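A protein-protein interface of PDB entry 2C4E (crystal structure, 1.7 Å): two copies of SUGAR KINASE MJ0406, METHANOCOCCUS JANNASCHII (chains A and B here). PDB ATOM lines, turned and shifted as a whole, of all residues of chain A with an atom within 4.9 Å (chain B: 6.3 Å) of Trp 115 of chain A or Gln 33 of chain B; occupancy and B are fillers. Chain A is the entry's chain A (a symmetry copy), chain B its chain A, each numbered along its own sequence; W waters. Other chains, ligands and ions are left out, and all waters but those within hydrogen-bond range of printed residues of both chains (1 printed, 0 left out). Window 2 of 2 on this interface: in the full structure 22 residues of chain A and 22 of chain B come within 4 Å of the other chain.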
ATOM      1  N   HIS A  13     -28.913  -6.775  -2.128  1.00  0.00           N
ATOM      2  CA  HIS A  13     -30.095  -7.382  -1.533  1.00  0.00           C
ATOM      3  C   HIS A  13     -31.411  -6.760  -1.964  1.00  0.00           C
ATOM      4  O   HIS A  13     -31.590  -5.547  -1.913  1.00  0.00           O
ATOM      5  CB  HIS A  13     -29.992  -7.308  -0.019  1.00  0.00           C
ATOM      6  CG  HIS A  13     -28.953  -8.216   0.552  1.00  0.00           C
ATOM      7  ND1 HIS A  13     -28.787  -9.518   0.128  1.00  0.00           N
ATOM      8  CD2 HIS A  13     -28.043  -8.018   1.532  1.00  0.00           C
ATOM      9  CE1 HIS A  13     -27.804 -10.076   0.814  1.00  0.00           C
ATOM     10  NE2 HIS A  13     -27.334  -9.187   1.669  1.00  0.00           N
ATOM     11  N   PRO A  97     -34.256 -13.544   0.583  1.00  0.00           N
ATOM     12  CA  PRO A  97     -33.671 -13.046   1.837  1.00  0.00           C
ATOM     13  C   PRO A  97     -34.666 -12.259   2.691  1.00  0.00           C
ATOM     14  O   PRO A  97     -35.502 -11.524   2.153  1.00  0.00           O
ATOM     15  CB  PRO A  97     -32.527 -12.133   1.356  1.00  0.00           C
ATOM     16  CG  PRO A  97     -32.118 -12.731   0.049  1.00  0.00           C
ATOM     17  CD  PRO A  97     -33.419 -13.192  -0.583  1.00  0.00           C
ATOM     18  N   PHE A 113     -30.711 -11.685   9.776  1.00  0.00           N
ATOM     19  CA  PHE A 113     -30.828 -11.660   8.315  1.00  0.00           C
ATOM     20  C   PHE A 113     -30.734 -13.066   7.716  1.00  0.00           C
ATOM     21  O   PHE A 113     -29.686 -13.708   7.774  1.00  0.00           O
ATOM     22  CB  PHE A 113     -29.762 -10.762   7.695  1.00  0.00           C
ATOM     23  CG  PHE A 113     -29.913 -10.592   6.211  1.00  0.00           C
ATOM     24  CD1 PHE A 113     -30.975  -9.863   5.690  1.00  0.00           C
ATOM     25  CD2 PHE A 113     -29.002 -11.172   5.330  1.00  0.00           C
ATOM     26  CE1 PHE A 113     -31.121  -9.703   4.318  1.00  0.00           C
ATOM     27  CE2 PHE A 113     -29.146 -11.016   3.965  1.00  0.00           C
ATOM     28  CZ  PHE A 113     -30.204 -10.283   3.454  1.00  0.00           C
ATOM     29  N   LEU A 114     -31.850 -13.557   7.182  1.00  0.00           N
ATOM     30  CA  LEU A 114     -31.883 -14.852   6.513  1.00  0.00           C
ATOM     31  C   LEU A 114     -31.259 -14.728   5.119  1.00  0.00           C
ATOM     32  O   LEU A 114     -31.818 -14.096   4.238  1.00  0.00           O
ATOM     33  CB  LEU A 114     -33.326 -15.363   6.417  1.00  0.00           C
ATOM     34  CG  LEU A 114     -33.531 -16.772   5.860  1.00  0.00           C
ATOM     35  CD1 LEU A 114     -32.773 -17.791   6.679  1.00  0.00           C
ATOM     36  CD2 LEU A 114     -35.013 -17.113   5.841  1.00  0.00           C
ATOM     37  N   TRP A 115     -30.110 -15.370   4.944  1.00  0.00           N
ATOM     38  CA  TRP A 115     -29.322 -15.314   3.709  1.00  0.00           C
ATOM     39  C   TRP A 115     -30.097 -15.865   2.509  1.00  0.00           C
ATOM     40  O   TRP A 115     -30.171 -15.221   1.470  1.00  0.00           O
ATOM     41  CB  TRP A 115     -28.046 -16.118   3.940  1.00  0.00           C
ATOM     42  CG  TRP A 115     -26.993 -16.003   2.906  1.00  0.00           C
ATOM     43  CD1 TRP A 115     -26.437 -17.032   2.214  1.00  0.00           C
ATOM     44  CD2 TRP A 115     -26.312 -14.816   2.486  1.00  0.00           C
ATOM     45  NE1 TRP A 115     -25.464 -16.560   1.372  1.00  0.00           N
ATOM     46  CE2 TRP A 115     -25.371 -15.199   1.513  1.00  0.00           C
ATOM     47  CE3 TRP A 115     -26.411 -13.460   2.817  1.00  0.00           C
ATOM     48  CZ2 TRP A 115     -24.536 -14.282   0.875  1.00  0.00           C
ATOM     49  CZ3 TRP A 115     -25.574 -12.551   2.184  1.00  0.00           C
ATOM     50  CH2 TRP A 115     -24.653 -12.968   1.226  1.00  0.00           C
ATOM     51  N   GLY A 116     -30.696 -17.049   2.677  1.00  0.00           N
ATOM     52  CA  GLY A 116     -31.554 -17.653   1.666  1.00  0.00           C
ATOM     53  C   GLY A 116     -30.930 -17.747   0.275  1.00  0.00           C
ATOM     54  O   GLY A 116     -29.853 -18.357   0.113  1.00  0.00           O
ATOM     55  N   ALA A 117     -31.601 -17.113  -0.703  1.00  0.00           N
ATOM     56  CA  ALA A 117     -31.203 -17.140  -2.124  1.00  0.00           C
ATOM     57  C   ALA A 117     -29.915 -16.380  -2.454  1.00  0.00           C
ATOM     58  O   ALA A 117     -29.362 -16.549  -3.543  1.00  0.00           O
ATOM     59  CB  ALA A 117     -32.346 -16.597  -2.995  1.00  0.00           C
ATOM     60  N   ALA A 118     -29.458 -15.519  -1.544  1.00  0.00           N
ATOM     61  CA  ALA A 118     -28.139 -14.889  -1.673  1.00  0.00           C
ATOM     62  C   ALA A 118     -26.989 -15.908  -1.752  1.00  0.00           C
ATOM     63  O   ALA A 118     -25.877 -15.570  -2.173  1.00  0.00           O
ATOM     64  CB  ALA A 118     -27.906 -13.920  -0.522  1.00  0.00           C
ATOM     65  N   LYS A 119     -27.246 -17.155  -1.359  1.00  0.00           N
ATOM     66  CA  LYS A 119     -26.255 -18.217  -1.547  1.00  0.00           C
ATOM     67  C   LYS A 119     -25.844 -18.353  -3.021  1.00  0.00           C
ATOM     68  O   LYS A 119     -24.759 -18.843  -3.323  1.00  0.00           O
ATOM     69  CB  LYS A 119     -26.749 -19.565  -0.978  1.00  0.00           C
ATOM     70  CG  LYS A 119     -27.881 -20.225  -1.760  1.00  0.00           C
ATOM     71  CD  LYS A 119     -27.364 -21.028  -2.939  1.00  0.00           C
ATOM     72  CE  LYS A 119     -28.039 -22.346  -3.090  1.00  0.00           C
ATOM     73  NZ  LYS A 119     -27.332 -23.222  -4.073  1.00  0.00           N
ATOM     74  N   GLY A 139     -24.603  -7.132   0.047  1.00  0.00           N
ATOM     75  CA  GLY A 139     -24.882  -8.312  -0.738  1.00  0.00           C
ATOM     76  C   GLY A 139     -23.829  -9.354  -0.472  1.00  0.00           C
ATOM     77  O   GLY A 139     -23.560  -9.694   0.691  1.00  0.00           O
ATOM     78  N   ASP A 140     -23.289  -9.919  -1.541  1.00  0.00           N
ATOM     79  CA  ASP A 140     -22.217 -10.891  -1.450  1.00  0.00           C
ATOM     80  C   ASP A 140     -20.937 -10.151  -1.819  1.00  0.00           C
ATOM     81  O   ASP A 140     -20.807  -9.665  -2.948  1.00  0.00           O
ATOM     82  CB  ASP A 140     -22.469 -12.037  -2.418  1.00  0.00           C
ATOM     83  CG  ASP A 140     -21.370 -13.055  -2.401  1.00  0.00           C
ATOM     84  OD1 ASP A 140     -21.470 -14.060  -1.658  1.00  0.00           O
ATOM     85  OD2 ASP A 140     -20.359 -12.939  -3.123  1.00  0.00           O
ATOM     86  N   ASN B  21     -30.126 -20.737  12.707  1.00  0.00           N
ATOM     87  CA  ASN B  21     -28.800 -21.006  13.264  1.00  0.00           C
ATOM     88  C   ASN B  21     -27.827 -19.838  13.063  1.00  0.00           C
ATOM     89  O   ASN B  21     -27.134 -19.757  12.047  1.00  0.00           O
ATOM     90  CB  ASN B  21     -28.222 -22.291  12.659  1.00  0.00           C
ATOM     91  CG  ASN B  21     -29.222 -23.435  12.637  1.00  0.00           C
ATOM     92  OD1 ASN B  21     -29.562 -24.002  13.676  1.00  0.00           O
ATOM     93  ND2 ASN B  21     -29.697 -23.780  11.445  1.00  0.00           N
ATOM     94  N   VAL B  22     -27.793 -18.937  14.045  1.00  0.00           N
ATOM     95  CA  VAL B  22     -26.918 -17.767  14.023  1.00  0.00           C
ATOM     96  C   VAL B  22     -25.613 -18.024  14.790  1.00  0.00           C
ATOM     97  O   VAL B  22     -25.508 -18.989  15.551  1.00  0.00           O
ATOM     98  CB  VAL B  22     -27.642 -16.511  14.601  1.00  0.00           C
ATOM     99  CG1 VAL B  22     -27.707 -16.543  16.129  1.00  0.00           C
ATOM    100  CG2 VAL B  22     -26.974 -15.230  14.116  1.00  0.00           C
ATOM    101  N   GLU B  23     -24.629 -17.150  14.582  1.00  0.00           N
ATOM    102  CA  GLU B  23     -23.342 -17.246  15.272  1.00  0.00           C
ATOM    103  C   GLU B  23     -23.419 -16.563  16.637  1.00  0.00           C
ATOM    104  O   GLU B  23     -23.289 -17.224  17.671  1.00  0.00           O
ATOM    105  CB  GLU B  23     -22.224 -16.621  14.429  1.00  0.00           C
ATOM    106  CG  GLU B  23     -21.842 -17.431  13.198  1.00  0.00           C
ATOM    107  CD  GLU B  23     -22.553 -16.962  11.943  1.00  0.00           C
ATOM    108  OE1 GLU B  23     -23.712 -17.374  11.724  1.00  0.00           O
ATOM    109  OE2 GLU B  23     -21.953 -16.182  11.174  1.00  0.00           O
ATOM    110  N   SER B  31     -25.380  -6.266  11.917  1.00  0.00           N
ATOM    111  CA  SER B  31     -26.099  -7.283  11.146  1.00  0.00           C
ATOM    112  C   SER B  31     -25.307  -8.587  11.025  1.00  0.00           C
ATOM    113  O   SER B  31     -24.362  -8.687  10.242  1.00  0.00           O
ATOM    114  CB  SER B  31     -26.438  -6.747   9.753  1.00  0.00           C
ATOM    115  OG  SER B  31     -27.188  -5.547   9.837  1.00  0.00           O
ATOM    116  N   ILE B  32     -25.847  -9.558  11.755  1.00  0.00           N
ATOM    117  CA  ILE B  32     -25.284 -10.911  11.694  1.00  0.00           C
ATOM    118  C   ILE B  32     -26.262 -11.702  10.837  1.00  0.00           C
ATOM    119  O   ILE B  32     -27.347 -11.194  10.538  1.00  0.00           O
ATOM    120  CB  ILE B  32     -25.042 -11.487  13.095  1.00  0.00           C
ATOM    121  CG1 ILE B  32     -24.161 -10.541  13.922  1.00  0.00           C
ATOM    122  CG2 ILE B  32     -24.406 -12.876  13.010  1.00  0.00           C
ATOM    123  CD1 ILE B  32     -24.170 -10.831  15.410  1.00  0.00           C
ATOM    124  N   GLN B  33     -25.881 -12.921  10.392  1.00  0.00           N
ATOM    125  CA  GLN B  33     -26.792 -13.670   9.522  1.00  0.00           C
ATOM    126  C   GLN B  33     -27.030 -15.136   9.883  1.00  0.00           C
ATOM    127  O   GLN B  33     -26.343 -15.726  10.724  1.00  0.00           O
ATOM    128  CB  GLN B  33     -26.325 -13.558   8.069  1.00  0.00           C
ATOM    129  CG  GLN B  33     -25.530 -14.748   7.535  1.00  0.00           C
ATOM    130  CD  GLN B  33     -24.942 -14.475   6.167  1.00  0.00           C
ATOM    131  OE1 GLN B  33     -25.023 -13.357   5.663  1.00  0.00           O
ATOM    132  NE2 GLN B  33     -24.360 -15.500   5.557  1.00  0.00           N
ATOM    133  N   ILE B  34     -28.030 -15.696   9.204  1.00  0.00           N
ATOM    134  CA  ILE B  34     -28.485 -17.070   9.351  1.00  0.00           C
ATOM    135  C   ILE B  34     -28.534 -17.673   7.941  1.00  0.00           C
ATOM    136  O   ILE B  34     -29.158 -17.093   7.060  1.00  0.00           O
ATOM    137  CB  ILE B  34     -29.893 -17.074   9.988  1.00  0.00           C
ATOM    138  CG1 ILE B  34     -29.988 -15.959  11.045  1.00  0.00           C
ATOM    139  CG2 ILE B  34     -30.203 -18.433  10.564  1.00  0.00           C
ATOM    140  CD1 ILE B  34     -31.191 -15.992  11.927  1.00  0.00           C
ATOM    141  N   PRO B  35     -27.892 -18.818   7.706  1.00  0.00           N
ATOM    142  CA  PRO B  35     -27.802 -19.361   6.340  1.00  0.00           C
ATOM    143  C   PRO B  35     -29.167 -19.775   5.783  1.00  0.00           C
ATOM    144  O   PRO B  35     -29.543 -19.401   4.675  1.00  0.00           O
ATOM    145  CB  PRO B  35     -26.871 -20.575   6.494  1.00  0.00           C
ATOM    146  CG  PRO B  35     -26.932 -20.948   7.935  1.00  0.00           C
ATOM    147  CD  PRO B  35     -27.228 -19.691   8.692  1.00  0.00           C
ATOM    148  N   SER B  36     -29.923 -20.523   6.568  1.00  0.00           N
ATOM    149  CA  SER B  36     -31.254 -20.938   6.184  1.00  0.00           C
ATOM    150  C   SER B  36     -32.063 -21.255   7.422  1.00  0.00           C
ATOM    151  O   SER B  36     -31.543 -21.292   8.537  1.00  0.00           O
ATOM    152  CB  SER B  36     -31.216 -22.115   5.207  1.00  0.00           C
ATOM    153  OG  SER B  36     -30.642 -23.260   5.811  1.00  0.00           O
HETATM  154  O   HOH W   1     -28.602 -20.016   2.204  1.00  0.00           O
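O of Phe 113 of chain A touches CB of Gln 33 of chain B, at 3.4 Å. Leu 114 of chain A touches Ile 34 of chain B. CA of Ser 36 of chain B touches CD1 of Leu 114 of chain A, 3.5 Å away. CE3 of Trp 115 of chain A touches OE1 of Gln 33 of chain B (3.2 Å). Trp 115 of chain A touches Pro 35 of chain B (CB to O, 3.7 Å).
Of the 9 printed residues of chain B, 5 touch a printed residue of chain A. Printed residues of chain A that touch a printed residue of chain B: Phe 113, Leu 114, Trp 115 and Gly 116. Among the printed residues, 9 pairs touch across the chains. Among the printed residues, no Asp or Glu carboxylate lies within 4 Å of a Lys or Arg side-chain nitrogen of the other chain.
Water W1 bridges the backbone carbonyl oxygen (O) of Pro 35 of chain B (2.7 Å) and the backbone carbonyl oxygen (O) of Gly 116 of chain A (2.9 Å).
O of Ile 34 of chain B sits at hydrogen-bond distance from N of Trp 115 of chain A. The backbone carbonyl oxygen (O) of Pro 35 of chain B is in hydrogen-bond range of the backbone NH (N) of Gly 116 of chain A (3.3 Å). The backbone NH (N) of Ile 34 of chain B is in hydrogen-bond range of the backbone carbonyl oxygen (O) of Phe 113 of chain A (3.0 Å). The backbone carbonyl oxygen of Ile 32 of chain B is in hydrogen-bond range of the backbone NH of Phe 113 of chain A, at 3.5 Å.
Trp 115 of chain A touches just these residues of chain B: Gln 33, Ile 34 and Pro 35. Gln 33 of chain B touches just these residues of chain A: Phe 113 and Trp 115. Of the printed residues of chain B, Gly 116 of chain A touches Pro 35. Printed residues of chain A within 4 Å of Ile 34 of chain B: Phe 113, Leu 114 and Trp 115. The nearest residue of chain B that does not touch Trp 115 of chain A is Ser 36 of chain B (5.4 Å). The nearest printed residue of chain B that does not touch Phe 113 of chain A is Pro 35 of chain B (5.4 Å).
No position is printed for both chains. Of the 9 pairs that touch across the chains among the printed residues, none has its exchanged pair printed and touching as well.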
